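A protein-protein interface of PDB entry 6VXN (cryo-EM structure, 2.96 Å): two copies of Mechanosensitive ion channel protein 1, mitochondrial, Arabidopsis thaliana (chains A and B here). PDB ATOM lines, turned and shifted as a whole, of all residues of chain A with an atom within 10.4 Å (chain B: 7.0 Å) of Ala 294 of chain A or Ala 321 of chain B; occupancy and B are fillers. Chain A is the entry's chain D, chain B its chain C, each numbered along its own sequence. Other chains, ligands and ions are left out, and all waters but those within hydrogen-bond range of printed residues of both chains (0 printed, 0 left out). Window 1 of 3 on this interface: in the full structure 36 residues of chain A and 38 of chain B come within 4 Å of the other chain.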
ATOM      1  N   THR A 271      19.070   2.849  30.693  1.00  0.00           N
ATOM      2  CA  THR A 271      19.889   3.021  29.504  1.00  0.00           C
ATOM      3  C   THR A 271      20.923   4.101  29.780  1.00  0.00           C
ATOM      4  O   THR A 271      20.566   5.250  30.044  1.00  0.00           O
ATOM      5  CB  THR A 271      19.032   3.403  28.304  1.00  0.00           C
ATOM      6  OG1 THR A 271      18.069   2.376  28.061  1.00  0.00           O
ATOM      7  CG2 THR A 271      19.895   3.566  27.081  1.00  0.00           C
ATOM      8  N   ILE A 272      22.198   3.735  29.735  1.00  0.00           N
ATOM      9  CA  ILE A 272      23.265   4.662  30.068  1.00  0.00           C
ATOM     10  C   ILE A 272      24.202   4.803  28.881  1.00  0.00           C
ATOM     11  O   ILE A 272      24.183   4.016  27.931  1.00  0.00           O
ATOM     12  CB  ILE A 272      24.061   4.229  31.314  1.00  0.00           C
ATOM     13  CG1 ILE A 272      24.909   3.002  30.999  1.00  0.00           C
ATOM     14  CG2 ILE A 272      23.147   3.948  32.471  1.00  0.00           C
ATOM     15  CD1 ILE A 272      26.024   2.781  31.970  1.00  0.00           C
ATOM     16  N   LYS A 273      25.017   5.850  28.945  1.00  0.00           N
ATOM     17  CA  LYS A 273      26.149   6.039  28.052  1.00  0.00           C
ATOM     18  C   LYS A 273      27.308   6.548  28.887  1.00  0.00           C
ATOM     19  O   LYS A 273      27.193   7.591  29.531  1.00  0.00           O
ATOM     20  CB  LYS A 273      25.824   7.022  26.932  1.00  0.00           C
ATOM     21  CG  LYS A 273      27.046   7.566  26.242  1.00  0.00           C
ATOM     22  CD  LYS A 273      26.693   8.668  25.284  1.00  0.00           C
ATOM     23  CE  LYS A 273      27.898   9.035  24.449  1.00  0.00           C
ATOM     24  NZ  LYS A 273      28.627   7.814  24.015  1.00  0.00           N
ATOM     25  N   SER A 276      32.734   5.368  25.905  1.00  0.00           N
ATOM     26  CA  SER A 276      32.664   4.541  24.710  1.00  0.00           C
ATOM     27  C   SER A 276      31.497   3.569  24.721  1.00  0.00           C
ATOM     28  O   SER A 276      31.045   3.163  23.646  1.00  0.00           O
ATOM     29  CB  SER A 276      33.966   3.757  24.536  1.00  0.00           C
ATOM     30  OG  SER A 276      34.303   3.058  25.720  1.00  0.00           O
ATOM     31  N   VAL A 277      31.000   3.188  25.890  1.00  0.00           N
ATOM     32  CA  VAL A 277      29.964   2.183  25.990  1.00  0.00           C
ATOM     33  C   VAL A 277      28.608   2.858  26.124  1.00  0.00           C
ATOM     34  O   VAL A 277      28.482   3.980  26.620  1.00  0.00           O
ATOM     35  CB  VAL A 277      30.218   1.214  27.160  1.00  0.00           C
ATOM     36  CG1 VAL A 277      31.498   0.488  26.930  1.00  0.00           C
ATOM     37  CG2 VAL A 277      30.280   1.959  28.468  1.00  0.00           C
ATOM     38  N   GLU A 278      27.573   2.142  25.688  1.00  0.00           N
ATOM     39  CA  GLU A 278      26.212   2.658  25.676  1.00  0.00           C
ATOM     40  C   GLU A 278      25.218   1.515  25.558  1.00  0.00           C
ATOM     41  O   GLU A 278      25.379   0.641  24.705  1.00  0.00           O
ATOM     42  CB  GLU A 278      26.033   3.640  24.519  1.00  0.00           C
ATOM     43  CG  GLU A 278      24.653   4.234  24.414  1.00  0.00           C
ATOM     44  CD  GLU A 278      24.492   5.075  23.173  1.00  0.00           C
ATOM     45  OE1 GLU A 278      23.483   4.894  22.459  1.00  0.00           O
ATOM     46  OE2 GLU A 278      25.377   5.914  22.908  1.00  0.00           O
ATOM     47  N   GLY A 279      24.199   1.504  26.401  1.00  0.00           N
ATOM     48  CA  GLY A 279      23.185   0.475  26.317  1.00  0.00           C
ATOM     49  C   GLY A 279      22.463   0.314  27.639  1.00  0.00           C
ATOM     50  O   GLY A 279      22.641   1.100  28.562  1.00  0.00           O
ATOM     51  N   GLN A 280      21.634  -0.722  27.695  1.00  0.00           N
ATOM     52  CA  GLN A 280      20.884  -1.018  28.906  1.00  0.00           C
ATOM     53  C   GLN A 280      21.762  -1.726  29.917  1.00  0.00           C
ATOM     54  O   GLN A 280      22.713  -2.412  29.561  1.00  0.00           O
ATOM     55  CB  GLN A 280      19.684  -1.907  28.611  1.00  0.00           C
ATOM     56  CG  GLN A 280      18.695  -1.334  27.656  1.00  0.00           C
ATOM     57  CD  GLN A 280      17.424  -2.133  27.654  1.00  0.00           C
ATOM     58  OE1 GLN A 280      16.839  -2.384  28.706  1.00  0.00           O
ATOM     59  NE2 GLN A 280      16.991  -2.558  26.474  1.00  0.00           N
ATOM     60  N   VAL A 281      21.413  -1.584  31.185  1.00  0.00           N
ATOM     61  CA  VAL A 281      22.147  -2.211  32.275  1.00  0.00           C
ATOM     62  C   VAL A 281      21.409  -3.487  32.651  1.00  0.00           C
ATOM     63  O   VAL A 281      20.308  -3.429  33.203  1.00  0.00           O
ATOM     64  CB  VAL A 281      22.275  -1.271  33.476  1.00  0.00           C
ATOM     65  CG1 VAL A 281      22.961  -1.969  34.603  1.00  0.00           C
ATOM     66  CG2 VAL A 281      23.030  -0.026  33.090  1.00  0.00           C
ATOM     67  N   LEU A 291      26.202  -4.682  30.093  1.00  0.00           N
ATOM     68  CA  LEU A 291      25.273  -3.870  29.332  1.00  0.00           C
ATOM     69  C   LEU A 291      24.763  -4.659  28.138  1.00  0.00           C
ATOM     70  O   LEU A 291      25.274  -5.721  27.794  1.00  0.00           O
ATOM     71  CB  LEU A 291      25.927  -2.572  28.852  1.00  0.00           C
ATOM     72  CG  LEU A 291      26.696  -1.686  29.822  1.00  0.00           C
ATOM     73  CD1 LEU A 291      27.010  -0.387  29.136  1.00  0.00           C
ATOM     74  CD2 LEU A 291      25.899  -1.433  31.070  1.00  0.00           C
ATOM     75  N   LEU A 292      23.749  -4.100  27.502  1.00  0.00           N
ATOM     76  CA  LEU A 292      23.170  -4.631  26.277  1.00  0.00           C
ATOM     77  C   LEU A 292      23.141  -3.468  25.302  1.00  0.00           C
ATOM     78  O   LEU A 292      22.381  -2.517  25.502  1.00  0.00           O
ATOM     79  CB  LEU A 292      21.770  -5.176  26.533  1.00  0.00           C
ATOM     80  CG  LEU A 292      21.182  -6.221  25.602  1.00  0.00           C
ATOM     81  CD1 LEU A 292      21.786  -7.560  25.916  1.00  0.00           C
ATOM     82  CD2 LEU A 292      19.689  -6.264  25.766  1.00  0.00           C
ATOM     83  N   ASN A 293      23.973  -3.518  24.266  1.00  0.00           N
ATOM     84  CA  ASN A 293      24.196  -2.348  23.424  1.00  0.00           C
ATOM     85  C   ASN A 293      23.066  -2.199  22.404  1.00  0.00           C
ATOM     86  O   ASN A 293      22.002  -2.808  22.525  1.00  0.00           O
ATOM     87  CB  ASN A 293      25.582  -2.410  22.788  1.00  0.00           C
ATOM     88  CG  ASN A 293      25.733  -3.540  21.808  1.00  0.00           C
ATOM     89  OD1 ASN A 293      25.000  -4.514  21.857  1.00  0.00           O
ATOM     90  ND2 ASN A 293      26.701  -3.422  20.917  1.00  0.00           N
ATOM     91  N   ALA A 294      23.282  -1.348  21.398  1.00  0.00           N
ATOM     92  CA  ALA A 294      22.222  -1.003  20.454  1.00  0.00           C
ATOM     93  C   ALA A 294      21.853  -2.163  19.541  1.00  0.00           C
ATOM     94  O   ALA A 294      20.722  -2.222  19.052  1.00  0.00           O
ATOM     95  CB  ALA A 294      22.637   0.201  19.616  1.00  0.00           C
ATOM     96  N   GLU A 295      22.775  -3.088  19.296  1.00  0.00           N
ATOM     97  CA  GLU A 295      22.484  -4.289  18.531  1.00  0.00           C
ATOM     98  C   GLU A 295      22.150  -5.471  19.421  1.00  0.00           C
ATOM     99  O   GLU A 295      22.128  -6.605  18.935  1.00  0.00           O
ATOM    100  CB  GLU A 295      23.657  -4.641  17.627  1.00  0.00           C
ATOM    101  CG  GLU A 295      23.873  -3.668  16.506  1.00  0.00           C
ATOM    102  CD  GLU A 295      25.094  -4.001  15.693  1.00  0.00           C
ATOM    103  OE1 GLU A 295      26.202  -4.006  16.268  1.00  0.00           O
ATOM    104  OE2 GLU A 295      24.951  -4.264  14.481  1.00  0.00           O
ATOM    105  N   LYS A 296      21.924  -5.221  20.715  1.00  0.00           N
ATOM    106  CA  LYS A 296      21.476  -6.203  21.705  1.00  0.00           C
ATOM    107  C   LYS A 296      22.495  -7.326  21.899  1.00  0.00           C
ATOM    108  O   LYS A 296      22.129  -8.481  22.108  1.00  0.00           O
ATOM    109  CB  LYS A 296      20.091  -6.763  21.368  1.00  0.00           C
ATOM    110  CG  LYS A 296      19.042  -5.700  21.090  1.00  0.00           C
ATOM    111  CD  LYS A 296      18.961  -4.683  22.204  1.00  0.00           C
ATOM    112  CE  LYS A 296      17.683  -3.884  22.130  1.00  0.00           C
ATOM    113  NZ  LYS A 296      17.814  -2.745  21.192  1.00  0.00           N
ATOM    114  N   PHE A 297      23.773  -6.981  21.833  1.00  0.00           N
ATOM    115  CA  PHE A 297      24.899  -7.832  22.198  1.00  0.00           C
ATOM    116  C   PHE A 297      25.287  -7.554  23.640  1.00  0.00           C
ATOM    117  O   PHE A 297      25.312  -6.392  24.050  1.00  0.00           O
ATOM    118  CB  PHE A 297      26.101  -7.555  21.315  1.00  0.00           C
ATOM    119  CG  PHE A 297      25.906  -7.892  19.875  1.00  0.00           C
ATOM    120  CD1 PHE A 297      25.212  -9.018  19.497  1.00  0.00           C
ATOM    121  CD2 PHE A 297      26.439  -7.080  18.894  1.00  0.00           C
ATOM    122  CE1 PHE A 297      25.050  -9.324  18.170  1.00  0.00           C
ATOM    123  CE2 PHE A 297      26.276  -7.380  17.569  1.00  0.00           C
ATOM    124  CZ  PHE A 297      25.582  -8.502  17.205  1.00  0.00           C
ATOM    125  N   PRO A 298      25.598  -8.570  24.447  1.00  0.00           N
ATOM    126  CA  PRO A 298      26.032  -8.305  25.826  1.00  0.00           C
ATOM    127  C   PRO A 298      27.464  -7.788  25.872  1.00  0.00           C
ATOM    128  O   PRO A 298      28.399  -8.467  25.446  1.00  0.00           O
ATOM    129  CB  PRO A 298      25.900  -9.672  26.505  1.00  0.00           C
ATOM    130  CG  PRO A 298      25.897 -10.641  25.411  1.00  0.00           C
ATOM    131  CD  PRO A 298      25.283  -9.987  24.234  1.00  0.00           C
ATOM    132  N   VAL A 299      27.627  -6.578  26.392  1.00  0.00           N
ATOM    133  CA  VAL A 299      28.924  -5.950  26.614  1.00  0.00           C
ATOM    134  C   VAL A 299      29.313  -6.164  28.067  1.00  0.00           C
ATOM    135  O   VAL A 299      28.457  -6.119  28.956  1.00  0.00           O
ATOM    136  CB  VAL A 299      28.863  -4.451  26.273  1.00  0.00           C
ATOM    137  CG1 VAL A 299      30.247  -3.861  26.146  1.00  0.00           C
ATOM    138  CG2 VAL A 299      28.085  -4.239  25.005  1.00  0.00           C
ATOM    139  N   LYS A 314      19.951   8.051  30.295  1.00  0.00           N
ATOM    140  CA  LYS A 314      18.837   8.353  29.410  1.00  0.00           C
ATOM    141  C   LYS A 314      17.490   7.900  29.947  1.00  0.00           C
ATOM    142  O   LYS A 314      16.474   8.167  29.304  1.00  0.00           O
ATOM    143  CB  LYS A 314      19.074   7.713  28.047  1.00  0.00           C
ATOM    144  CG  LYS A 314      20.433   8.006  27.465  1.00  0.00           C
ATOM    145  CD  LYS A 314      20.651   7.216  26.202  1.00  0.00           C
ATOM    146  CE  LYS A 314      21.685   7.867  25.327  1.00  0.00           C
ATOM    147  NZ  LYS A 314      22.782   8.410  26.151  1.00  0.00           N
ATOM    148  N   LYS A 385       9.143   4.733  24.354  1.00  0.00           N
ATOM    149  CA  LYS A 385       9.847   4.844  23.085  1.00  0.00           C
ATOM    150  C   LYS A 385       8.952   4.627  21.873  1.00  0.00           C
ATOM    151  O   LYS A 385       9.406   4.857  20.752  1.00  0.00           O
ATOM    152  CB  LYS A 385      11.005   3.851  23.047  1.00  0.00           C
ATOM    153  CG  LYS A 385      12.302   4.425  22.517  1.00  0.00           C
ATOM    154  CD  LYS A 385      13.352   3.337  22.394  1.00  0.00           C
ATOM    155  CE  LYS A 385      14.598   3.841  21.691  1.00  0.00           C
ATOM    156  NZ  LYS A 385      15.638   2.780  21.597  1.00  0.00           N
ATOM    157  N   TYR A 389       8.104   8.010  18.995  1.00  0.00           N
ATOM    158  CA  TYR A 389       8.150   7.905  17.541  1.00  0.00           C
ATOM    159  C   TYR A 389       6.833   8.336  16.911  1.00  0.00           C
ATOM    160  O   TYR A 389       6.827   9.042  15.888  1.00  0.00           O
ATOM    161  CB  TYR A 389       8.487   6.475  17.139  1.00  0.00           C
ATOM    162  CG  TYR A 389       9.899   6.061  17.462  1.00  0.00           C
ATOM    163  CD1 TYR A 389      10.919   6.999  17.527  1.00  0.00           C
ATOM    164  CD2 TYR A 389      10.215   4.732  17.681  1.00  0.00           C
ATOM    165  CE1 TYR A 389      12.212   6.620  17.816  1.00  0.00           C
ATOM    166  CE2 TYR A 389      11.501   4.346  17.972  1.00  0.00           C
ATOM    167  CZ  TYR A 389      12.494   5.293  18.036  1.00  0.00           C
ATOM    168  OH  TYR A 389      13.779   4.909  18.322  1.00  0.00           O
ATOM    169  N   TRP B 319      18.150 -12.322  21.843  1.00  0.00           N
ATOM    170  CA  TRP B 319      17.330 -11.752  20.788  1.00  0.00           C
ATOM    171  C   TRP B 319      18.175 -10.718  20.067  1.00  0.00           C
ATOM    172  O   TRP B 319      19.158 -10.215  20.608  1.00  0.00           O
ATOM    173  CB  TRP B 319      16.032 -11.139  21.325  1.00  0.00           C
ATOM    174  CG  TRP B 319      16.193 -10.072  22.352  1.00  0.00           C
ATOM    175  CD1 TRP B 319      16.326  -8.739  22.129  1.00  0.00           C
ATOM    176  CD2 TRP B 319      16.197 -10.241  23.771  1.00  0.00           C
ATOM    177  NE1 TRP B 319      16.431  -8.067  23.318  1.00  0.00           N
ATOM    178  CE2 TRP B 319      16.355  -8.971  24.342  1.00  0.00           C
ATOM    179  CE3 TRP B 319      16.090 -11.348  24.614  1.00  0.00           C
ATOM    180  CZ2 TRP B 319      16.411  -8.776  25.712  1.00  0.00           C
ATOM    181  CZ3 TRP B 319      16.146 -11.153  25.971  1.00  0.00           C
ATOM    182  CH2 TRP B 319      16.306  -9.878  26.508  1.00  0.00           C
ATOM    183  N   ARG B 320      17.791 -10.419  18.836  1.00  0.00           N
ATOM    184  CA  ARG B 320      18.544  -9.519  17.977  1.00  0.00           C
ATOM    185  C   ARG B 320      17.671  -8.337  17.603  1.00  0.00           C
ATOM    186  O   ARG B 320      16.459  -8.472  17.486  1.00  0.00           O
ATOM    187  CB  ARG B 320      19.014 -10.232  16.717  1.00  0.00           C
ATOM    188  CG  ARG B 320      19.969 -11.364  16.984  1.00  0.00           C
ATOM    189  CD  ARG B 320      21.331 -10.825  17.343  1.00  0.00           C
ATOM    190  NE  ARG B 320      21.907 -10.062  16.244  1.00  0.00           N
ATOM    191  CZ  ARG B 320      22.679 -10.586  15.301  1.00  0.00           C
ATOM    192  NH1 ARG B 320      22.966 -11.878  15.326  1.00  0.00           N
ATOM    193  NH2 ARG B 320      23.163  -9.821  14.334  1.00  0.00           N
ATOM    194  N   ALA B 321      18.279  -7.175  17.431  1.00  0.00           N
ATOM    195  CA  ALA B 321      17.549  -5.984  17.033  1.00  0.00           C
ATOM    196  C   ALA B 321      17.833  -5.679  15.574  1.00  0.00           C
ATOM    197  O   ALA B 321      18.992  -5.507  15.189  1.00  0.00           O
ATOM    198  CB  ALA B 321      17.932  -4.792  17.901  1.00  0.00           C
ATOM    199  N   ILE B 322      16.783  -5.612  14.761  1.00  0.00           N
ATOM    200  CA  ILE B 322      16.940  -5.229  13.365  1.00  0.00           C
ATOM    201  C   ILE B 322      16.168  -3.943  13.115  1.00  0.00           C
ATOM    202  O   ILE B 322      15.191  -3.625  13.804  1.00  0.00           O
ATOM    203  CB  ILE B 322      16.502  -6.343  12.384  1.00  0.00           C
ATOM    204  CG1 ILE B 322      14.984  -6.483  12.325  1.00  0.00           C
ATOM    205  CG2 ILE B 322      17.138  -7.660  12.751  1.00  0.00           C
ATOM    206  CD1 ILE B 322      14.502  -7.337  11.191  1.00  0.00           C
ATOM    207  N   ALA B 323      16.647  -3.186  12.130  1.00  0.00           N
ATOM    208  CA  ALA B 323      16.048  -1.922  11.736  1.00  0.00           C
ATOM    209  C   ALA B 323      16.402  -1.640  10.286  1.00  0.00           C
ATOM    210  O   ALA B 323      17.358  -2.194   9.742  1.00  0.00           O
ATOM    211  CB  ALA B 323      16.521  -0.771  12.625  1.00  0.00           C
ATOM    212  N   GLU B 358      10.562  -4.750  23.695  1.00  0.00           N
ATOM    213  CA  GLU B 358      10.208  -3.576  22.914  1.00  0.00           C
ATOM    214  C   GLU B 358       9.184  -3.947  21.857  1.00  0.00           C
ATOM    215  O   GLU B 358       9.325  -4.964  21.174  1.00  0.00           O
ATOM    216  CB  GLU B 358      11.432  -2.958  22.240  1.00  0.00           C
ATOM    217  CG  GLU B 358      12.237  -2.035  23.123  1.00  0.00           C
ATOM    218  CD  GLU B 358      13.544  -2.650  23.570  1.00  0.00           C
ATOM    219  OE1 GLU B 358      13.823  -3.804  23.185  1.00  0.00           O
ATOM    220  OE2 GLU B 358      14.294  -1.975  24.306  1.00  0.00           O
ATOM    221  N   GLY B 377      11.584  -1.140  12.702  1.00  0.00           N
ATOM    222  CA  GLY B 377      12.456  -1.918  13.552  1.00  0.00           C
ATOM    223  C   GLY B 377      11.733  -2.873  14.469  1.00  0.00           C
ATOM    224  O   GLY B 377      10.593  -2.624  14.866  1.00  0.00           O
ATOM    225  N   CYS B 378      12.410  -3.960  14.825  1.00  0.00           N
ATOM    226  CA  CYS B 378      11.838  -4.959  15.719  1.00  0.00           C
ATOM    227  C   CYS B 378      12.965  -5.769  16.337  1.00  0.00           C
ATOM    228  O   CYS B 378      14.143  -5.576  16.029  1.00  0.00           O
ATOM    229  CB  CYS B 378      10.851  -5.865  14.981  1.00  0.00           C
ATOM    230  SG  CYS B 378      11.495  -6.633  13.487  1.00  0.00           S
ATOM    231  N   ASN B 379      12.590  -6.665  17.244  1.00  0.00           N
ATOM    232  CA  ASN B 379      13.497  -7.637  17.833  1.00  0.00           C
ATOM    233  C   ASN B 379      13.111  -9.019  17.337  1.00  0.00           C
ATOM    234  O   ASN B 379      11.977  -9.454  17.535  1.00  0.00           O
ATOM    235  CB  ASN B 379      13.441  -7.609  19.361  1.00  0.00           C
ATOM    236  CG  ASN B 379      14.018  -6.345  19.955  1.00  0.00           C
ATOM    237  OD1 ASN B 379      13.874  -6.093  21.145  1.00  0.00           O
ATOM    238  ND2 ASN B 379      14.689  -5.552  19.136  1.00  0.00           N
ATOM    239  N   LEU B 380      14.051  -9.702  16.706  1.00  0.00           N
ATOM    240  CA  LEU B 380      13.871 -11.085  16.312  1.00  0.00           C
ATOM    241  C   LEU B 380      14.369 -12.010  17.412  1.00  0.00           C
ATOM    242  O   LEU B 380      15.236 -11.648  18.203  1.00  0.00           O
ATOM    243  CB  LEU B 380      14.620 -11.386  15.017  1.00  0.00           C
ATOM    244  CG  LEU B 380      14.482 -10.411  13.859  1.00  0.00           C
ATOM    245  CD1 LEU B 380      15.300 -10.917  12.701  1.00  0.00           C
ATOM    246  CD2 LEU B 380      13.041 -10.278  13.462  1.00  0.00           C
ATOM    247  N   LEU B 388      18.502 -15.213  10.087  1.00  0.00           N
ATOM    248  CA  LEU B 388      18.544 -13.769  10.301  1.00  0.00           C
ATOM    249  C   LEU B 388      18.451 -13.009   8.987  1.00  0.00           C
ATOM    250  O   LEU B 388      17.653 -12.075   8.853  1.00  0.00           O
ATOM    251  CB  LEU B 388      19.822 -13.396  11.044  1.00  0.00           C
ATOM    252  CG  LEU B 388      19.967 -11.943  11.485  1.00  0.00           C
ATOM    253  CD1 LEU B 388      19.044 -11.648  12.641  1.00  0.00           C
ATOM    254  CD2 LEU B 388      21.396 -11.640  11.858  1.00  0.00           C
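No position is printed for both chains.
Printed residues of chain B that touch a printed residue of chain A: Trp 319, Arg 320, Ala 321 and Glu 358.
Hydrophobic or aromatic side chains of chain B within 4 Å of the printed part of chain A: Ala 321.
Ala 294 of chain A touches one residue of chain B.
Of the printed residues of chain B, Lys 296 of chain A touches Trp 319 (3.7 Å) and Ala 321 (3.5 Å).
Printed residues of chain B within 4 Å of Phe 297 of chain A: Arg 320.
Ala 321 of chain B touches just these residues of chain A: Ala 294 and Lys 296.
Of the printed residues of chain A, Glu 358 of chain B touches Gln 280.
The nearest residue of chain B that does not touch Ala 294 of chain A is Ile 322 of chain B (6.7 Å).
The nearest residue of chain A that does not touch Ala 321 of chain B is Glu 295 of chain A (4.2 Å).
Gln 280 of chain A touches Glu 358 of chain B.
CB of Ala 321 of chain B touches O of Ala 294 of chain A, 3.96 Å away.
Trp 319 of chain B touches Lys 296 of chain A.
Lys 296 of chain A touches Ala 321 of chain B (CG to CB, 3.5 Å).
Arg 320 of chain B touches Phe 297 of chain A.
O of Arg 320 of chain B is in hydrogen-bond range of N of Leu 380 of chain B (2.8 Å).
The side-chain amide oxygen (OD1) of Asn 379 of chain B sits close to the side-chain carboxylate (OE1) of Glu 358 of chain B, 3.1 Å away.
The backbone NH of Leu 292 of chain A is in hydrogen-bond range of the backbone carbonyl oxygen of Gln 280 of chain A, 2.9 Å away.
OD1 of Asn 293 of chain A lies within hydrogen-bond range of N of Lys 296 of chain A.
The side-chain amide oxygen (OD1) of Asn 293 of chain A sits at hydrogen-bond distance from the backbone NH (N) of Phe 297 of chain A (2.8 Å).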
